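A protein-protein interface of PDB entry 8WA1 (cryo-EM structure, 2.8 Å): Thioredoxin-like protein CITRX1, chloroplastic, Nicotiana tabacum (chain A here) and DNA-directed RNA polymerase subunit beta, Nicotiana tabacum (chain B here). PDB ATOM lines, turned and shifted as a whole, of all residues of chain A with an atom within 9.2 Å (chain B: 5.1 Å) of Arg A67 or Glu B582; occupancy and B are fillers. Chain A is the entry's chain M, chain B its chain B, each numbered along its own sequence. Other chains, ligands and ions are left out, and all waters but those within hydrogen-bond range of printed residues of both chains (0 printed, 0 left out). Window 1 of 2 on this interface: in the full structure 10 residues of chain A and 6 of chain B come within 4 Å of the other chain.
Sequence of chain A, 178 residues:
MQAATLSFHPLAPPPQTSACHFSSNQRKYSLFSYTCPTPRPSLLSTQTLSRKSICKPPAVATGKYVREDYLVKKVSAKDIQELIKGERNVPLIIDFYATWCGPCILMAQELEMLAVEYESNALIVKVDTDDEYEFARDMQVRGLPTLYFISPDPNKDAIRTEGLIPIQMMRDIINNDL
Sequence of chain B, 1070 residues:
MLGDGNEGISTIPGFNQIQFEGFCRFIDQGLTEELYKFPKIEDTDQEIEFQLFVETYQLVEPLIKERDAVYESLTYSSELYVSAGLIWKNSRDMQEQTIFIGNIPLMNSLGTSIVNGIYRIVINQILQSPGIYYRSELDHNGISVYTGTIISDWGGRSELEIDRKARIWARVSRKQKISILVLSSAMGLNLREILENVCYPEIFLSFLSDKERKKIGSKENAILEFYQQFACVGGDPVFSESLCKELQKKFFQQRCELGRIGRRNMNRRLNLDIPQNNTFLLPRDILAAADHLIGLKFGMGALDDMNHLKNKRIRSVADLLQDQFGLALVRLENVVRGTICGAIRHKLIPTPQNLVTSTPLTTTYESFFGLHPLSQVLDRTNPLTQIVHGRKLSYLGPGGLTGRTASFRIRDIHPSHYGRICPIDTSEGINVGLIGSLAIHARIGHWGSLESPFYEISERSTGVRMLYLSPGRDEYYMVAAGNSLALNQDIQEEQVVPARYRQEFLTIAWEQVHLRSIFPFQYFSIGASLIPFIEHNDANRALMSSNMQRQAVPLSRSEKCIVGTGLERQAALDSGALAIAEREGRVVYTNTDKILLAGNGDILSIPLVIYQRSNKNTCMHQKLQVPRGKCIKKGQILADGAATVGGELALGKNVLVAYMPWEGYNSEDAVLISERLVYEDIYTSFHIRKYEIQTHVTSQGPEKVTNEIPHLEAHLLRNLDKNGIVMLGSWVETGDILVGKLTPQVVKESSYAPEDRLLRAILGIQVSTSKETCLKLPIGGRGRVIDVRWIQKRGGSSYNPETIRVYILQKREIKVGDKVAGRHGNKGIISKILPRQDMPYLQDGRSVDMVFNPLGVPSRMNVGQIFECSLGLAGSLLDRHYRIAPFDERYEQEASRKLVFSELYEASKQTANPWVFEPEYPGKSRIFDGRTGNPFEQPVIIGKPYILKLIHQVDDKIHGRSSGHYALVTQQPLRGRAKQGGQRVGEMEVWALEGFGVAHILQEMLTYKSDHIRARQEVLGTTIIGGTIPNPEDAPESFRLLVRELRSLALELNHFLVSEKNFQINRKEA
The side-chain carboxylate (OE2) of Glu B584 is in salt-bridge range of the guanidinium group (NE) of Arg A67 (2.6 Å).
OD1 of Asp A69 is in salt-bridge range of NZ of Lys B634.
OE1 of Glu A68 lies within salt-bridge range of NH1 of Arg A67, 3.9 Å away.
Among the printed residues, pairs that only touch across the chains: Arg A67 with Glu B582 (3.7 Å), Arg A67 with Lys B634 (3.2 Å), Glu A68 with Glu B584 (3.98 Å) and Leu A71 with Glu B584 (3.7 Å).
Of the printed residues of chain B, Arg A67 touches Glu B582 (3.7 Å), Glu B584 (2.6 Å) and Lys B634 (3.2 Å).
Glu B582 touches just one residue of chain A: Arg A67 (3.7 Å).
Printed residues of chain A within 4 Å of Glu B584: Arg A67, Glu A68 and Leu A71.
Of the printed residues of chain B, Asp A69 touches Lys B634 (3.3 Å).
Printed residues of chain A within 4 Å of Lys B634: Arg A67 (3.2 Å) and Asp A69 (3.3 Å).
Printed residues of chain B within 4 Å of Leu A71: Glu B584 (3.7 Å).
Asn B600 touches none of the printed residues of chain A.
The nearest residue of chain A that does not touch Glu B582 is Val A66 (5.9 Å).
The nearest printed residue of chain A that does not touch Glu B584 is Val A116 (4.2 Å).
Printed residues of chain B that touch a printed residue of chain A: Glu B582, Glu B584 and Lys B634.
Of the 14 printed residues of chain A, 4 touch a printed residue of chain B.
Hydrophobic or aromatic side chains of chain A within 4 Å of the printed part of chain B: Leu A71.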
ATOM      1  N   GLY A  63      14.348 -23.449  -0.310  1.00  0.00           N
ATOM      2  CA  GLY A  63      15.371 -23.529   0.716  1.00  0.00           C
ATOM      3  C   GLY A  63      15.524 -24.923   1.292  1.00  0.00           C
ATOM      4  O   GLY A  63      16.237 -25.125   2.275  1.00  0.00           O
ATOM      5  N   LYS A  64      14.845 -25.890   0.674  1.00  0.00           N
ATOM      6  CA  LYS A  64      14.923 -27.269   1.146  1.00  0.00           C
ATOM      7  C   LYS A  64      16.266 -27.897   0.796  1.00  0.00           C
ATOM      8  O   LYS A  64      16.897 -28.549   1.635  1.00  0.00           O
ATOM      9  CB  LYS A  64      13.773 -28.085   0.554  1.00  0.00           C
ATOM     10  CG  LYS A  64      13.825 -29.570   0.875  1.00  0.00           C
ATOM     11  CD  LYS A  64      12.690 -30.315   0.190  1.00  0.00           C
ATOM     12  CE  LYS A  64      12.778 -31.813   0.435  1.00  0.00           C
ATOM     13  NZ  LYS A  64      11.706 -32.552  -0.288  1.00  0.00           N
ATOM     14  N   TYR A  65      16.722 -27.704  -0.443  1.00  0.00           N
ATOM     15  CA  TYR A  65      17.945 -28.360  -0.894  1.00  0.00           C
ATOM     16  C   TYR A  65      19.185 -27.639  -0.377  1.00  0.00           C
ATOM     17  O   TYR A  65      20.141 -28.278   0.077  1.00  0.00           O
ATOM     18  CB  TYR A  65      17.955 -28.443  -2.421  1.00  0.00           C
ATOM     19  CG  TYR A  65      16.861 -29.325  -2.978  1.00  0.00           C
ATOM     20  CD1 TYR A  65      16.637 -30.595  -2.464  1.00  0.00           C
ATOM     21  CD2 TYR A  65      16.038 -28.882  -4.005  1.00  0.00           C
ATOM     22  CE1 TYR A  65      15.636 -31.404  -2.965  1.00  0.00           C
ATOM     23  CE2 TYR A  65      15.032 -29.683  -4.512  1.00  0.00           C
ATOM     24  CZ  TYR A  65      14.835 -30.944  -3.988  1.00  0.00           C
ATOM     25  OH  TYR A  65      13.836 -31.746  -4.488  1.00  0.00           O
ATOM     26  N   VAL A  66      19.195 -26.310  -0.442  1.00  0.00           N
ATOM     27  CA  VAL A  66      20.323 -25.504   0.011  1.00  0.00           C
ATOM     28  C   VAL A  66      19.886 -24.696   1.225  1.00  0.00           C
ATOM     29  O   VAL A  66      18.822 -24.065   1.210  1.00  0.00           O
ATOM     30  CB  VAL A  66      20.858 -24.585  -1.104  1.00  0.00           C
ATOM     31  CG1 VAL A  66      21.601 -25.401  -2.146  1.00  0.00           C
ATOM     32  CG2 VAL A  66      19.722 -23.807  -1.753  1.00  0.00           C
ATOM     33  N   ARG A  67      20.699 -24.731   2.277  1.00  0.00           N
ATOM     34  CA  ARG A  67      20.398 -23.977   3.487  1.00  0.00           C
ATOM     35  C   ARG A  67      20.764 -22.509   3.300  1.00  0.00           C
ATOM     36  O   ARG A  67      21.697 -22.172   2.565  1.00  0.00           O
ATOM     37  CB  ARG A  67      21.156 -24.567   4.676  1.00  0.00           C
ATOM     38  CG  ARG A  67      20.782 -23.970   6.023  1.00  0.00           C
ATOM     39  CD  ARG A  67      19.305 -24.169   6.321  1.00  0.00           C
ATOM     40  NE  ARG A  67      18.919 -23.574   7.597  1.00  0.00           N
ATOM     41  CZ  ARG A  67      17.681 -23.581   8.080  1.00  0.00           C
ATOM     42  NH1 ARG A  67      16.703 -24.154   7.392  1.00  0.00           N
ATOM     43  NH2 ARG A  67      17.419 -23.014   9.250  1.00  0.00           N
ATOM     44  N   GLU A  68      20.018 -21.632   3.967  1.00  0.00           N
ATOM     45  CA  GLU A  68      20.299 -20.204   3.896  1.00  0.00           C
ATOM     46  C   GLU A  68      21.580 -19.876   4.654  1.00  0.00           C
ATOM     47  O   GLU A  68      21.840 -20.418   5.732  1.00  0.00           O
ATOM     48  CB  GLU A  68      19.131 -19.397   4.467  1.00  0.00           C
ATOM     49  CG  GLU A  68      17.882 -19.393   3.597  1.00  0.00           C
ATOM     50  CD  GLU A  68      17.112 -20.698   3.660  1.00  0.00           C
ATOM     51  OE1 GLU A  68      17.404 -21.521   4.551  1.00  0.00           O
ATOM     52  OE2 GLU A  68      16.214 -20.900   2.817  1.00  0.00           O
ATOM     53  N   ASP A  69      22.383 -18.979   4.079  1.00  0.00           N
ATOM     54  CA  ASP A  69      23.660 -18.631   4.693  1.00  0.00           C
ATOM     55  C   ASP A  69      23.469 -17.763   5.930  1.00  0.00           C
ATOM     56  O   ASP A  69      24.172 -17.937   6.932  1.00  0.00           O
ATOM     57  CB  ASP A  69      24.552 -17.923   3.671  1.00  0.00           C
ATOM     58  CG  ASP A  69      24.811 -18.769   2.439  1.00  0.00           C
ATOM     59  OD1 ASP A  69      24.318 -19.917   2.387  1.00  0.00           O
ATOM     60  OD2 ASP A  69      25.506 -18.287   1.521  1.00  0.00           O
ATOM     61  N   TYR A  70      22.529 -16.824   5.880  1.00  0.00           N
ATOM     62  CA  TYR A  70      22.291 -15.881   6.965  1.00  0.00           C
ATOM     63  C   TYR A  70      20.942 -16.176   7.606  1.00  0.00           C
ATOM     64  O   TYR A  70      19.948 -16.389   6.902  1.00  0.00           O
ATOM     65  CB  TYR A  70      22.344 -14.442   6.450  1.00  0.00           C
ATOM     66  CG  TYR A  70      23.618 -14.123   5.695  1.00  0.00           C
ATOM     67  CD1 TYR A  70      24.748 -13.671   6.361  1.00  0.00           C
ATOM     68  CD2 TYR A  70      23.691 -14.281   4.316  1.00  0.00           C
ATOM     69  CE1 TYR A  70      25.914 -13.383   5.677  1.00  0.00           C
ATOM     70  CE2 TYR A  70      24.852 -13.994   3.623  1.00  0.00           C
ATOM     71  CZ  TYR A  70      25.960 -13.545   4.309  1.00  0.00           C
ATOM     72  OH  TYR A  70      27.120 -13.257   3.627  1.00  0.00           O
ATOM     73  N   LEU A  71      20.909 -16.185   8.938  1.00  0.00           N
ATOM     74  CA  LEU A  71      19.717 -16.555   9.691  1.00  0.00           C
ATOM     75  C   LEU A  71      19.004 -15.366  10.320  1.00  0.00           C
ATOM     76  O   LEU A  71      17.949 -15.550  10.934  1.00  0.00           O
ATOM     77  CB  LEU A  71      20.075 -17.571  10.782  1.00  0.00           C
ATOM     78  CG  LEU A  71      20.157 -19.052  10.398  1.00  0.00           C
ATOM     79  CD1 LEU A  71      21.330 -19.336   9.469  1.00  0.00           C
ATOM     80  CD2 LEU A  71      20.241 -19.914  11.649  1.00  0.00           C
ATOM     81  N   VAL A  72      19.544 -14.157  10.186  1.00  0.00           N
ATOM     82  CA  VAL A  72      18.927 -12.952  10.729  1.00  0.00           C
ATOM     83  C   VAL A  72      18.236 -12.212   9.593  1.00  0.00           C
ATOM     84  O   VAL A  72      18.849 -11.950   8.551  1.00  0.00           O
ATOM     85  CB  VAL A  72      19.966 -12.057  11.425  1.00  0.00           C
ATOM     86  CG1 VAL A  72      19.332 -10.749  11.861  1.00  0.00           C
ATOM     87  CG2 VAL A  72      20.572 -12.778  12.618  1.00  0.00           C
ATOM     88  N   LYS A  73      16.965 -11.875   9.790  1.00  0.00           N
ATOM     89  CA  LYS A  73      16.145 -11.251   8.763  1.00  0.00           C
ATOM     90  C   LYS A  73      16.020  -9.754   9.014  1.00  0.00           C
ATOM     91  O   LYS A  73      15.987  -9.298  10.161  1.00  0.00           O
ATOM     92  CB  LYS A  73      14.752 -11.887   8.712  1.00  0.00           C
ATOM     93  CG  LYS A  73      14.765 -13.398   8.542  1.00  0.00           C
ATOM     94  CD  LYS A  73      15.516 -13.812   7.286  1.00  0.00           C
ATOM     95  CE  LYS A  73      15.561 -15.324   7.139  1.00  0.00           C
ATOM     96  NZ  LYS A  73      16.326 -15.743   5.932  1.00  0.00           N
ATOM     97  N   ALA A 115      22.580 -16.215  17.006  1.00  0.00           N
ATOM     98  CA  ALA A 115      21.397 -16.822  16.407  1.00  0.00           C
ATOM     99  C   ALA A 115      21.605 -18.311  16.171  1.00  0.00           C
ATOM    100  O   ALA A 115      20.664 -19.104  16.290  1.00  0.00           O
ATOM    101  CB  ALA A 115      21.048 -16.113  15.099  1.00  0.00           C
ATOM    102  N   VAL A 116      22.830 -18.709  15.822  1.00  0.00           N
ATOM    103  CA  VAL A 116      23.124 -20.132  15.682  1.00  0.00           C
ATOM    104  C   VAL A 116      23.063 -20.823  17.039  1.00  0.00           C
ATOM    105  O   VAL A 116      22.533 -21.934  17.163  1.00  0.00           O
ATOM    106  CB  VAL A 116      24.491 -20.335  14.999  1.00  0.00           C
ATOM    107  CG1 VAL A 116      24.862 -21.805  14.982  1.00  0.00           C
ATOM    108  CG2 VAL A 116      24.459 -19.788  13.581  1.00  0.00           C
ATOM    109  N   GLU A 119      18.784 -21.366  18.490  1.00  0.00           N
ATOM    110  CA  GLU A 119      18.077 -21.695  17.256  1.00  0.00           C
ATOM    111  C   GLU A 119      16.625 -21.227  17.303  1.00  0.00           C
ATOM    112  O   GLU A 119      16.170 -20.499  16.412  1.00  0.00           O
ATOM    113  CB  GLU A 119      18.157 -23.200  16.982  1.00  0.00           C
ATOM    114  CG  GLU A 119      17.915 -24.094  18.192  1.00  0.00           C
ATOM    115  CD  GLU A 119      19.174 -24.353  18.998  1.00  0.00           C
ATOM    116  OE1 GLU A 119      20.257 -23.894  18.579  1.00  0.00           O
ATOM    117  OE2 GLU A 119      19.079 -25.018  20.051  1.00  0.00           O
ATOM    118  N   ILE B 580      33.818 -28.708   5.033  1.00  0.00           N
ATOM    119  CA  ILE B 580      33.086 -27.472   5.273  1.00  0.00           C
ATOM    120  C   ILE B 580      31.615 -27.813   5.461  1.00  0.00           C
ATOM    121  O   ILE B 580      31.022 -28.512   4.631  1.00  0.00           O
ATOM    122  CB  ILE B 580      33.281 -26.461   4.127  1.00  0.00           C
ATOM    123  CG1 ILE B 580      33.122 -27.144   2.767  1.00  0.00           C
ATOM    124  CG2 ILE B 580      34.645 -25.797   4.233  1.00  0.00           C
ATOM    125  CD1 ILE B 580      33.304 -26.209   1.590  1.00  0.00           C
ATOM    126  N   ALA B 581      31.035 -27.332   6.558  1.00  0.00           N
ATOM    127  CA  ALA B 581      29.642 -27.625   6.854  1.00  0.00           C
ATOM    128  C   ALA B 581      28.721 -26.935   5.856  1.00  0.00           C
ATOM    129  O   ALA B 581      28.973 -25.809   5.416  1.00  0.00           O
ATOM    130  CB  ALA B 581      29.294 -27.186   8.277  1.00  0.00           C
ATOM    131  N   GLU B 582      27.639 -27.625   5.499  1.00  0.00           N
ATOM    132  CA  GLU B 582      26.615 -27.083   4.617  1.00  0.00           C
ATOM    133  C   GLU B 582      25.346 -26.705   5.370  1.00  0.00           C
ATOM    134  O   GLU B 582      24.314 -26.453   4.741  1.00  0.00           O
ATOM    135  CB  GLU B 582      26.290 -28.082   3.504  1.00  0.00           C
ATOM    136  CG  GLU B 582      27.469 -28.423   2.606  1.00  0.00           C
ATOM    137  CD  GLU B 582      27.099 -29.387   1.494  1.00  0.00           C
ATOM    138  OE1 GLU B 582      25.926 -29.813   1.441  1.00  0.00           O
ATOM    139  OE2 GLU B 582      27.979 -29.718   0.673  1.00  0.00           O
ATOM    140  N   ARG B 583      25.401 -26.657   6.699  1.00  0.00           N
ATOM    141  CA  ARG B 583      24.234 -26.356   7.514  1.00  0.00           C
ATOM    142  C   ARG B 583      24.704 -25.919   8.892  1.00  0.00           C
ATOM    143  O   ARG B 583      25.712 -26.414   9.402  1.00  0.00           O
ATOM    144  CB  ARG B 583      23.304 -27.570   7.626  1.00  0.00           C
ATOM    145  CG  ARG B 583      21.957 -27.279   8.266  1.00  0.00           C
ATOM    146  CD  ARG B 583      21.205 -28.565   8.576  1.00  0.00           C
ATOM    147  NE  ARG B 583      21.131 -29.456   7.422  1.00  0.00           N
ATOM    148  CZ  ARG B 583      20.155 -29.435   6.521  1.00  0.00           C
ATOM    149  NH1 ARG B 583      19.161 -28.565   6.636  1.00  0.00           N
ATOM    150  NH2 ARG B 583      20.170 -30.285   5.503  1.00  0.00           N
ATOM    151  N   GLU B 584      23.971 -24.983   9.486  1.00  0.00           N
ATOM    152  CA  GLU B 584      24.286 -24.550  10.837  1.00  0.00           C
ATOM    153  C   GLU B 584      23.720 -25.536  11.856  1.00  0.00           C
ATOM    154  O   GLU B 584      22.710 -26.206  11.622  1.00  0.00           O
ATOM    155  CB  GLU B 584      23.739 -23.145  11.102  1.00  0.00           C
ATOM    156  CG  GLU B 584      22.220 -23.050  11.149  1.00  0.00           C
ATOM    157  CD  GLU B 584      21.583 -23.074   9.773  1.00  0.00           C
ATOM    158  OE1 GLU B 584      22.319 -22.935   8.773  1.00  0.00           O
ATOM    159  OE2 GLU B 584      20.348 -23.234   9.691  1.00  0.00           O
ATOM    160  N   ASN B 600      18.451 -27.472  13.448  1.00  0.00           N
ATOM    161  CA  ASN B 600      17.026 -27.264  13.154  1.00  0.00           C
ATOM    162  C   ASN B 600      16.234 -28.571  13.191  1.00  0.00           C
ATOM    163  O   ASN B 600      15.396 -28.843  12.327  1.00  0.00           O
ATOM    164  CB  ASN B 600      16.831 -26.535  11.816  1.00  0.00           C
ATOM    165  CG  ASN B 600      17.441 -27.275  10.638  1.00  0.00           C
ATOM    166  OD1 ASN B 600      16.806 -28.139  10.033  1.00  0.00           O
ATOM    167  ND2 ASN B 600      18.677 -26.929  10.299  1.00  0.00           N
ATOM    168  N   LYS B 634      27.280 -22.185   8.355  1.00  0.00           N
ATOM    169  CA  LYS B 634      27.313 -22.803   7.032  1.00  0.00           C
ATOM    170  C   LYS B 634      28.504 -22.229   6.275  1.00  0.00           C
ATOM    171  O   LYS B 634      28.409 -21.164   5.661  1.00  0.00           O
ATOM    172  CB  LYS B 634      26.006 -22.562   6.287  1.00  0.00           C
ATOM    173  CG  LYS B 634      25.970 -23.180   4.901  1.00  0.00           C
ATOM    174  CD  LYS B 634      24.676 -22.859   4.178  1.00  0.00           C
ATOM    175  CE  LYS B 634      24.689 -23.421   2.768  1.00  0.00           C
ATOM    176  NZ  LYS B 634      25.813 -22.863   1.968  1.00  0.00           N
